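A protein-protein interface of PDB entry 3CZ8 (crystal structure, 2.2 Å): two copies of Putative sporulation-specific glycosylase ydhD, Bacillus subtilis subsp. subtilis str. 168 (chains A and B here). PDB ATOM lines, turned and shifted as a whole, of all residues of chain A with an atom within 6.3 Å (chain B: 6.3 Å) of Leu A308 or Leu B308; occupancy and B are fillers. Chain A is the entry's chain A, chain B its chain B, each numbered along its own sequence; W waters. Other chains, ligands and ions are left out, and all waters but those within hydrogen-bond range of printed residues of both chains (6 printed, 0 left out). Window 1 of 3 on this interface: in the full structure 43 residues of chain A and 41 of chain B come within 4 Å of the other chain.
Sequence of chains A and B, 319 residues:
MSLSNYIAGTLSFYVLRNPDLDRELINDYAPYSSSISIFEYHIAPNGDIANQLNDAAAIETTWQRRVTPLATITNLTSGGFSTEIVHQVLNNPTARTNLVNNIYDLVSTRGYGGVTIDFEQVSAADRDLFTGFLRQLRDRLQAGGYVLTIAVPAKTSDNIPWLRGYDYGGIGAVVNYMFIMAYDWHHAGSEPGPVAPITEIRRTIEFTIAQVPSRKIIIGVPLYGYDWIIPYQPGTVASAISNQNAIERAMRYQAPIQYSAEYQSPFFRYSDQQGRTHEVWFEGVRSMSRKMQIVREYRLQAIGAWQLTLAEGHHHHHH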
ATOM      1  N   GLY A   9     -26.240 -27.106   6.723  1.00  0.00           N
ATOM      2  CA  GLY A   9     -25.075 -26.270   6.465  1.00  0.00           C
ATOM      3  C   GLY A   9     -24.386 -25.826   7.739  1.00  0.00           C
ATOM      4  O   GLY A   9     -25.017 -25.247   8.626  1.00  0.00           O
ATOM      5  N   THR A  10     -23.091 -26.114   7.833  1.00  0.00           N
ATOM      6  CA  THR A  10     -22.260 -25.604   8.919  1.00  0.00           C
ATOM      7  C   THR A  10     -21.714 -24.227   8.535  1.00  0.00           C
ATOM      8  O   THR A  10     -20.992 -24.088   7.540  1.00  0.00           O
ATOM      9  CB  THR A  10     -21.094 -26.563   9.250  1.00  0.00           C
ATOM     10  OG1 THR A  10     -21.612 -27.864   9.559  1.00  0.00           O
ATOM     11  CG2 THR A  10     -20.279 -26.047  10.440  1.00  0.00           C
ATOM     12  N   LEU A  11     -22.075 -23.213   9.316  1.00  0.00           N
ATOM     13  CA  LEU A  11     -21.563 -21.868   9.096  1.00  0.00           C
ATOM     14  C   LEU A  11     -20.217 -21.686   9.789  1.00  0.00           C
ATOM     15  O   LEU A  11     -20.034 -22.086  10.937  1.00  0.00           O
ATOM     16  CB  LEU A  11     -22.561 -20.806   9.579  1.00  0.00           C
ATOM     17  CG  LEU A  11     -22.237 -19.336   9.284  1.00  0.00           C
ATOM     18  CD1 LEU A  11     -22.399 -19.017   7.795  1.00  0.00           C
ATOM     19  CD2 LEU A  11     -23.100 -18.411  10.125  1.00  0.00           C
ATOM     20  N   SER A  12     -19.276 -21.089   9.070  1.00  0.00           N
ATOM     21  CA  SER A  12     -18.021 -20.686   9.665  1.00  0.00           C
ATOM     22  C   SER A  12     -17.521 -19.360   9.099  1.00  0.00           C
ATOM     23  O   SER A  12     -17.784 -19.028   7.941  1.00  0.00           O
ATOM     24  CB  SER A  12     -16.970 -21.793   9.528  1.00  0.00           C
ATOM     25  OG  SER A  12     -16.525 -21.929   8.196  1.00  0.00           O
ATOM     26  N   LEU A 223     -22.851 -11.201   4.922  1.00  0.00           N
ATOM     27  CA  LEU A 223     -23.331 -12.533   4.596  1.00  0.00           C
ATOM     28  C   LEU A 223     -24.536 -12.430   3.650  1.00  0.00           C
ATOM     29  O   LEU A 223     -24.647 -13.208   2.702  1.00  0.00           O
ATOM     30  CB  LEU A 223     -23.694 -13.275   5.892  1.00  0.00           C
ATOM     31  CG  LEU A 223     -24.335 -14.670   5.924  1.00  0.00           C
ATOM     32  CD1 LEU A 223     -23.563 -15.720   5.126  1.00  0.00           C
ATOM     33  CD2 LEU A 223     -24.517 -15.110   7.375  1.00  0.00           C
ATOM     34  N   TYR A 224     -25.408 -11.447   3.897  1.00  0.00           N
ATOM     35  CA  TYR A 224     -26.694 -11.280   3.197  1.00  0.00           C
ATOM     36  C   TYR A 224     -26.807  -9.966   2.422  1.00  0.00           C
ATOM     37  O   TYR A 224     -26.351  -8.928   2.904  1.00  0.00           O
ATOM     38  CB  TYR A 224     -27.850 -11.265   4.209  1.00  0.00           C
ATOM     39  CG  TYR A 224     -28.110 -12.538   4.984  1.00  0.00           C
ATOM     40  CD1 TYR A 224     -28.499 -13.709   4.335  1.00  0.00           C
ATOM     41  CD2 TYR A 224     -28.026 -12.551   6.380  1.00  0.00           C
ATOM     42  CE1 TYR A 224     -28.760 -14.872   5.048  1.00  0.00           C
ATOM     43  CE2 TYR A 224     -28.288 -13.712   7.107  1.00  0.00           C
ATOM     44  CZ  TYR A 224     -28.653 -14.868   6.432  1.00  0.00           C
ATOM     45  OH  TYR A 224     -28.914 -16.022   7.133  1.00  0.00           O
ATOM     46  N   ALA A 240     -33.930 -11.719   3.001  1.00  0.00           N
ATOM     47  CA  ALA A 240     -32.489 -11.876   3.182  1.00  0.00           C
ATOM     48  C   ALA A 240     -31.968 -12.924   2.210  1.00  0.00           C
ATOM     49  O   ALA A 240     -32.299 -14.110   2.318  1.00  0.00           O
ATOM     50  CB  ALA A 240     -32.174 -12.279   4.622  1.00  0.00           C
ATOM     51  N   SER A 242     -28.559 -14.259  -0.550  1.00  0.00           N
ATOM     52  CA  SER A 242     -27.118 -14.257  -0.771  1.00  0.00           C
ATOM     53  C   SER A 242     -26.786 -13.321  -1.925  1.00  0.00           C
ATOM     54  O   SER A 242     -27.673 -12.910  -2.675  1.00  0.00           O
ATOM     55  CB  SER A 242     -26.593 -15.679  -1.040  1.00  0.00           C
ATOM     56  OG  SER A 242     -26.733 -16.046  -2.408  1.00  0.00           O
ATOM     57  N   ASN A 245     -27.743 -14.976  -5.073  1.00  0.00           N
ATOM     58  CA  ASN A 245     -29.209 -14.869  -5.186  1.00  0.00           C
ATOM     59  C   ASN A 245     -29.684 -13.554  -5.784  1.00  0.00           C
ATOM     60  O   ASN A 245     -30.629 -13.541  -6.567  1.00  0.00           O
ATOM     61  CB  ASN A 245     -29.896 -15.043  -3.835  1.00  0.00           C
ATOM     62  CG  ASN A 245     -29.792 -16.443  -3.291  1.00  0.00           C
ATOM     63  OD1 ASN A 245     -29.967 -16.649  -2.093  1.00  0.00           O
ATOM     64  ND2 ASN A 245     -29.521 -17.417  -4.159  1.00  0.00           N
ATOM     65  N   TRP A 306     -17.578 -15.482   4.900  1.00  0.00           N
ATOM     66  CA  TRP A 306     -18.386 -16.628   5.327  1.00  0.00           C
ATOM     67  C   TRP A 306     -18.331 -17.809   4.367  1.00  0.00           C
ATOM     68  O   TRP A 306     -18.264 -17.636   3.152  1.00  0.00           O
ATOM     69  CB  TRP A 306     -19.841 -16.197   5.508  1.00  0.00           C
ATOM     70  CG  TRP A 306     -20.011 -15.030   6.429  1.00  0.00           C
ATOM     71  CD1 TRP A 306     -20.036 -13.702   6.084  1.00  0.00           C
ATOM     72  CD2 TRP A 306     -20.184 -15.079   7.849  1.00  0.00           C
ATOM     73  NE1 TRP A 306     -20.214 -12.928   7.205  1.00  0.00           N
ATOM     74  CE2 TRP A 306     -20.306 -13.747   8.302  1.00  0.00           C
ATOM     75  CE3 TRP A 306     -20.250 -16.123   8.786  1.00  0.00           C
ATOM     76  CZ2 TRP A 306     -20.493 -13.430   9.651  1.00  0.00           C
ATOM     77  CZ3 TRP A 306     -20.430 -15.806  10.124  1.00  0.00           C
ATOM     78  CH2 TRP A 306     -20.551 -14.466  10.544  1.00  0.00           C
ATOM     79  N   GLN A 307     -18.367 -19.013   4.929  1.00  0.00           N
ATOM     80  CA  GLN A 307     -18.469 -20.235   4.134  1.00  0.00           C
ATOM     81  C   GLN A 307     -19.472 -21.202   4.757  1.00  0.00           C
ATOM     82  O   GLN A 307     -19.649 -21.233   5.981  1.00  0.00           O
ATOM     83  CB  GLN A 307     -17.097 -20.898   3.952  1.00  0.00           C
ATOM     84  CG  GLN A 307     -16.247 -20.917   5.206  1.00  0.00           C
ATOM     85  CD  GLN A 307     -14.919 -21.636   5.041  1.00  0.00           C
ATOM     86  OE1 GLN A 307     -14.367 -21.722   3.942  1.00  0.00           O
ATOM     87  NE2 GLN A 307     -14.390 -22.147   6.148  1.00  0.00           N
ATOM     88  N   LEU A 308     -20.141 -21.967   3.903  1.00  0.00           N
ATOM     89  CA  LEU A 308     -21.077 -22.998   4.338  1.00  0.00           C
ATOM     90  C   LEU A 308     -20.568 -24.351   3.881  1.00  0.00           C
ATOM     91  O   LEU A 308     -20.303 -24.546   2.694  1.00  0.00           O
ATOM     92  CB  LEU A 308     -22.475 -22.759   3.761  1.00  0.00           C
ATOM     93  CG  LEU A 308     -23.473 -21.795   4.421  1.00  0.00           C
ATOM     94  CD1 LEU A 308     -23.705 -22.129   5.902  1.00  0.00           C
ATOM     95  CD2 LEU A 308     -23.105 -20.314   4.226  1.00  0.00           C
ATOM     96  N   THR A 309     -20.428 -25.278   4.823  1.00  0.00           N
ATOM     97  CA  THR A 309     -19.928 -26.613   4.509  1.00  0.00           C
ATOM     98  C   THR A 309     -20.955 -27.682   4.876  1.00  0.00           C
ATOM     99  O   THR A 309     -21.293 -27.865   6.049  1.00  0.00           O
ATOM    100  CB  THR A 309     -18.555 -26.879   5.175  1.00  0.00           C
ATOM    101  OG1 THR A 309     -17.597 -25.941   4.663  1.00  0.00           O
ATOM    102  CG2 THR A 309     -18.064 -28.294   4.886  1.00  0.00           C
ATOM    103  N   LEU A 310     -21.447 -28.370   3.849  1.00  0.00           N
ATOM    104  CA  LEU A 310     -22.447 -29.427   3.993  1.00  0.00           C
ATOM    105  C   LEU A 310     -21.778 -30.746   4.374  1.00  0.00           C
ATOM    106  O   LEU A 310     -20.816 -31.174   3.731  1.00  0.00           O
ATOM    107  CB  LEU A 310     -23.240 -29.585   2.690  1.00  0.00           C
ATOM    108  CG  LEU A 310     -24.542 -28.806   2.444  1.00  0.00           C
ATOM    109  CD1 LEU A 310     -24.403 -27.294   2.593  1.00  0.00           C
ATOM    110  CD2 LEU A 310     -25.073 -29.145   1.059  1.00  0.00           C
ATOM    111  N   ALA B   8     -28.067 -23.680  11.721  1.00  0.00           N
ATOM    112  CA  ALA B   8     -28.060 -24.808  10.798  1.00  0.00           C
ATOM    113  C   ALA B   8     -28.692 -24.384   9.479  1.00  0.00           C
ATOM    114  O   ALA B   8     -29.849 -23.952   9.444  1.00  0.00           O
ATOM    115  CB  ALA B   8     -28.798 -25.995  11.399  1.00  0.00           C
ATOM    116  N   GLY B   9     -27.924 -24.507   8.400  1.00  0.00           N
ATOM    117  CA  GLY B   9     -28.355 -24.045   7.086  1.00  0.00           C
ATOM    118  C   GLY B   9     -29.271 -24.995   6.340  1.00  0.00           C
ATOM    119  O   GLY B   9     -28.882 -26.121   6.022  1.00  0.00           O
ATOM    120  N   THR B  10     -30.489 -24.533   6.063  1.00  0.00           N
ATOM    121  CA  THR B  10     -31.459 -25.299   5.280  1.00  0.00           C
ATOM    122  C   THR B  10     -31.257 -25.045   3.791  1.00  0.00           C
ATOM    123  O   THR B  10     -31.377 -23.913   3.312  1.00  0.00           O
ATOM    124  CB  THR B  10     -32.921 -24.970   5.665  1.00  0.00           C
ATOM    125  OG1 THR B  10     -33.074 -25.041   7.088  1.00  0.00           O
ATOM    126  CG2 THR B  10     -33.892 -25.947   4.998  1.00  0.00           C
ATOM    127  N   LEU B  11     -30.947 -26.115   3.069  1.00  0.00           N
ATOM    128  CA  LEU B  11     -30.744 -26.053   1.636  1.00  0.00           C
ATOM    129  C   LEU B  11     -32.093 -26.127   0.943  1.00  0.00           C
ATOM    130  O   LEU B  11     -32.949 -26.937   1.312  1.00  0.00           O
ATOM    131  CB  LEU B  11     -29.890 -27.236   1.181  1.00  0.00           C
ATOM    132  CG  LEU B  11     -28.775 -27.105   0.137  1.00  0.00           C
ATOM    133  CD1 LEU B  11     -28.810 -28.323  -0.782  1.00  0.00           C
ATOM    134  CD2 LEU B  11     -28.790 -25.791  -0.658  1.00  0.00           C
ATOM    135  N   SER B  12     -32.285 -25.269  -0.052  1.00  0.00           N
ATOM    136  CA  SER B  12     -33.443 -25.378  -0.921  1.00  0.00           C
ATOM    137  C   SER B  12     -33.088 -25.033  -2.362  1.00  0.00           C
ATOM    138  O   SER B  12     -32.211 -24.201  -2.624  1.00  0.00           O
ATOM    139  CB  SER B  12     -34.621 -24.534  -0.410  1.00  0.00           C
ATOM    140  OG  SER B  12     -34.383 -23.148  -0.585  1.00  0.00           O
ATOM    141  N   TYR B 224     -21.477 -25.434  -5.986  1.00  0.00           N
ATOM    142  CA  TYR B 224     -20.074 -25.223  -5.685  1.00  0.00           C
ATOM    143  C   TYR B 224     -19.152 -25.083  -6.886  1.00  0.00           C
ATOM    144  O   TYR B 224     -19.395 -25.615  -7.980  1.00  0.00           O
ATOM    145  CB  TYR B 224     -19.566 -26.272  -4.689  1.00  0.00           C
ATOM    146  CG  TYR B 224     -20.224 -26.149  -3.330  1.00  0.00           C
ATOM    147  CD1 TYR B 224     -20.079 -24.990  -2.567  1.00  0.00           C
ATOM    148  CD2 TYR B 224     -20.999 -27.187  -2.811  1.00  0.00           C
ATOM    149  CE1 TYR B 224     -20.685 -24.865  -1.322  1.00  0.00           C
ATOM    150  CE2 TYR B 224     -21.610 -27.072  -1.561  1.00  0.00           C
ATOM    151  CZ  TYR B 224     -21.447 -25.907  -0.825  1.00  0.00           C
ATOM    152  OH  TYR B 224     -22.045 -25.780   0.407  1.00  0.00           O
ATOM    153  N   ALA B 240     -14.236 -27.842  -2.147  1.00  0.00           N
ATOM    154  CA  ALA B 240     -15.532 -27.383  -2.640  1.00  0.00           C
ATOM    155  C   ALA B 240     -15.874 -26.042  -2.017  1.00  0.00           C
ATOM    156  O   ALA B 240     -16.179 -25.959  -0.826  1.00  0.00           O
ATOM    157  CB  ALA B 240     -16.618 -28.407  -2.339  1.00  0.00           C
ATOM    158  N   SER B 242     -17.867 -22.005  -2.445  1.00  0.00           N
ATOM    159  CA  SER B 242     -18.946 -21.271  -3.100  1.00  0.00           C
ATOM    160  C   SER B 242     -18.361 -20.343  -4.162  1.00  0.00           C
ATOM    161  O   SER B 242     -17.150 -20.105  -4.190  1.00  0.00           O
ATOM    162  CB  SER B 242     -19.791 -20.494  -2.082  1.00  0.00           C
ATOM    163  OG  SER B 242     -19.163 -19.282  -1.701  1.00  0.00           O
ATOM    164  N   ASN B 245     -16.896 -17.483  -2.431  1.00  0.00           N
ATOM    165  CA  ASN B 245     -15.619 -17.954  -1.869  1.00  0.00           C
ATOM    166  C   ASN B 245     -14.470 -17.951  -2.880  1.00  0.00           C
ATOM    167  O   ASN B 245     -13.316 -17.716  -2.508  1.00  0.00           O
ATOM    168  CB  ASN B 245     -15.749 -19.364  -1.270  1.00  0.00           C
ATOM    169  CG  ASN B 245     -16.582 -19.408   0.005  1.00  0.00           C
ATOM    170  OD1 ASN B 245     -17.079 -20.470   0.379  1.00  0.00           O
ATOM    171  ND2 ASN B 245     -16.732 -18.268   0.681  1.00  0.00           N
ATOM    172  N   TRP B 306     -29.794 -22.383  -5.998  1.00  0.00           N
ATOM    173  CA  TRP B 306     -29.766 -22.782  -4.609  1.00  0.00           C
ATOM    174  C   TRP B 306     -29.888 -21.605  -3.653  1.00  0.00           C
ATOM    175  O   TRP B 306     -29.329 -20.528  -3.886  1.00  0.00           O
ATOM    176  CB  TRP B 306     -28.501 -23.587  -4.311  1.00  0.00           C
ATOM    177  CG  TRP B 306     -28.304 -24.733  -5.237  1.00  0.00           C
ATOM    178  CD1 TRP B 306     -27.581 -24.737  -6.403  1.00  0.00           C
ATOM    179  CD2 TRP B 306     -28.842 -26.053  -5.093  1.00  0.00           C
ATOM    180  NE1 TRP B 306     -27.637 -25.978  -6.990  1.00  0.00           N
ATOM    181  CE2 TRP B 306     -28.406 -26.804  -6.211  1.00  0.00           C
ATOM    182  CE3 TRP B 306     -29.655 -26.675  -4.134  1.00  0.00           C
ATOM    183  CZ2 TRP B 306     -28.744 -28.154  -6.388  1.00  0.00           C
ATOM    184  CZ3 TRP B 306     -29.999 -28.017  -4.316  1.00  0.00           C
ATOM    185  CH2 TRP B 306     -29.541 -28.740  -5.435  1.00  0.00           C
ATOM    186  N   GLN B 307     -30.650 -21.837  -2.590  1.00  0.00           N
ATOM    187  CA  GLN B 307     -30.814 -20.911  -1.485  1.00  0.00           C
ATOM    188  C   GLN B 307     -30.328 -21.599  -0.226  1.00  0.00           C
ATOM    189  O   GLN B 307     -30.491 -22.816  -0.070  1.00  0.00           O
ATOM    190  CB  GLN B 307     -32.285 -20.572  -1.289  1.00  0.00           C
ATOM    191  CG  GLN B 307     -32.805 -19.430  -2.125  1.00  0.00           C
ATOM    192  CD  GLN B 307     -34.313 -19.261  -1.999  1.00  0.00           C
ATOM    193  OE1 GLN B 307     -35.026 -20.192  -1.611  1.00  0.00           O
ATOM    194  NE2 GLN B 307     -34.806 -18.073  -2.331  1.00  0.00           N
ATOM    195  N   LEU B 308     -29.744 -20.812   0.671  1.00  0.00           N
ATOM    196  CA  LEU B 308     -29.335 -21.295   1.983  1.00  0.00           C
ATOM    197  C   LEU B 308     -29.997 -20.450   3.070  1.00  0.00           C
ATOM    198  O   LEU B 308     -29.752 -19.246   3.170  1.00  0.00           O
ATOM    199  CB  LEU B 308     -27.809 -21.258   2.110  1.00  0.00           C
ATOM    200  CG  LEU B 308     -27.084 -22.160   3.120  1.00  0.00           C
ATOM    201  CD1 LEU B 308     -27.229 -21.641   4.549  1.00  0.00           C
ATOM    202  CD2 LEU B 308     -27.504 -23.633   3.010  1.00  0.00           C
ATOM    203  N   THR B 309     -30.836 -21.093   3.878  1.00  0.00           N
ATOM    204  CA  THR B 309     -31.551 -20.417   4.958  1.00  0.00           C
ATOM    205  C   THR B 309     -31.132 -20.988   6.313  1.00  0.00           C
ATOM    206  O   THR B 309     -31.570 -22.074   6.698  1.00  0.00           O
ATOM    207  CB  THR B 309     -33.086 -20.539   4.782  1.00  0.00           C
ATOM    208  OG1 THR B 309     -33.447 -20.202   3.436  1.00  0.00           O
ATOM    209  CG2 THR B 309     -33.820 -19.612   5.750  1.00  0.00           C
ATOM    210  N   LEU B 310     -30.280 -20.259   7.031  1.00  0.00           N
ATOM    211  CA  LEU B 310     -29.837 -20.702   8.356  1.00  0.00           C
ATOM    212  C   LEU B 310     -30.704 -20.137   9.481  1.00  0.00           C
ATOM    213  O   LEU B 310     -30.829 -18.920   9.641  1.00  0.00           O
ATOM    214  CB  LEU B 310     -28.336 -20.437   8.581  1.00  0.00           C
ATOM    215  CG  LEU B 310     -27.677 -19.115   8.189  1.00  0.00           C
ATOM    216  CD1 LEU B 310     -27.537 -18.188   9.382  1.00  0.00           C
ATOM    217  CD2 LEU B 310     -26.321 -19.377   7.557  1.00  0.00           C
HETATM  218  O   HOH W   1     -32.977 -16.195  -2.589  1.00  0.00           O
HETATM  219  O   HOH W   2     -18.531 -15.599   1.789  1.00  0.00           O
HETATM  220  O   HOH W   3     -28.578 -18.273  -0.191  1.00  0.00           O
HETATM  221  O   HOH W   4     -20.075 -17.633   0.424  1.00  0.00           O
HETATM  222  O   HOH W   5     -19.347 -21.916   1.130  1.00  0.00           O
HETATM  223  O   HOH W   6     -18.088 -24.777   1.140  1.00  0.00           O
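Water W2 bridges O of Trp A306 (2.5 Å) and ND2 of Asn B245 (3.4 Å). Water W1 bridges the side-chain amide nitrogen of Gln B307 (2.6 Å) and the side-chain amide oxygen of Asn A245 (3.1 Å). Water W6 lies within hydrogen-bond range of O of Leu A308 (2.7 Å) and O of Ala B240 (3.0 Å). Water W5 lies within hydrogen-bond range of the side-chain amide oxygen of Asn B245 (2.8 Å) and the backbone NH of Leu A308 (2.9 Å). Water W4 lies within hydrogen-bond range of OG of Ser B242 (2.8 Å), O of Trp A306 (3.3 Å) and ND2 of Asn B245 (3.4 Å). Water W3 lies within hydrogen-bond range of the side-chain amide oxygen (OD1) of Asn A245 (2.9 Å) and the backbone NH (N) of Leu B308 (2.9 Å).
Printed residues of chain B that touch a printed residue of chain A: Ala B8, Gly B9, Tyr B224, Asn B245, Trp B306, Gln B307, Leu B308 and Leu B310. Hydrophobic or aromatic side chains of chain B within 4 Å of the printed part of chain A: Tyr B224, Leu B308 and Leu B310. Hydrophobic or aromatic side chains of chain A within 4 Å of the printed part of chain B: Leu A11, Tyr A224, Leu A308 and Leu A310.
Printed residues of chain B within 4 Å of Leu A308: Tyr B224 and Leu B308. Of the printed residues of chain A, Leu B308 touches Leu A308. Of the printed residues of chain A, Gly B9 touches Gly A9 (2.9 Å). Of the printed residues of chain B, Gln A307 touches Asn B245. Printed residues of chain A within 4 Å of Leu B310: Leu A11 (3.9 Å) and Tyr A224 (3.4 Å). Of the printed residues of chain A, Asn B245 touches Trp A306 (3.0 Å) and Gln A307 (3.6 Å). The nearest printed residue of chain A that does not touch Leu B308 is Leu A310 (4.8 Å). The nearest printed residue of chain B that does not touch Tyr A224 is Leu B308 (4.9 Å).
ND2 of Asn A245 is in hydrogen-bond range of O of Trp B306. The backbone carbonyl oxygen (O) of Trp A306 lies within hydrogen-bond range of the side-chain amide nitrogen (ND2) of Asn B245 (3.0 Å). The backbone carbonyl oxygen (O) of Gly B9 sits at hydrogen-bond distance from the backbone NH (N) of Gly A9 (2.9 Å). The side-chain hydroxyl (OH) of Tyr B224 sits at hydrogen-bond distance from the backbone carbonyl oxygen (O) of Leu A308 (3.1 Å).
Gly A9 touches its own counterpart, Gly B9. Tyr A224 touches Leu B310, and with the chains exchanged Leu A310 touches Tyr B224. Leu A308 touches Tyr B224, but with the chains exchanged Tyr A224 does not touch Leu B308 (4.9 Å). Leu B308 touches its own counterpart, Leu A308. Positions printed for both chains: 9, 10, 11, 12, 224, 240, 242, 245, 306, 307, 308, 309 and 310.
Gly A9 touches Ala B8. Leu B310 touches Leu A11. Tyr A224 touches Leu B310 (OH to CD1, 3.4 Å). Asn A245 touches Gln B307 (OD1 to CG, 3.97 Å). Gln A307 touches Asn B245 (CB to OD1, 3.6 Å). Leu A308 touches Leu B308. Leu A310 touches Tyr B224.
NE2 of Gln A307 sits at hydrogen-bond distance from OG of Ser A12 (3.0 Å). The side-chain hydroxyl (OG) of Ser B242 lies within hydrogen-bond range of the backbone NH (N) of Asn B245, 3.0 Å away. N of Gln B307 is in hydrogen-bond range of O of Ser B12 (2.8 Å). The side-chain hydroxyl (OG) of Ser A242 sits at hydrogen-bond distance from the backbone NH (N) of Asn A245 (3.0 Å).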
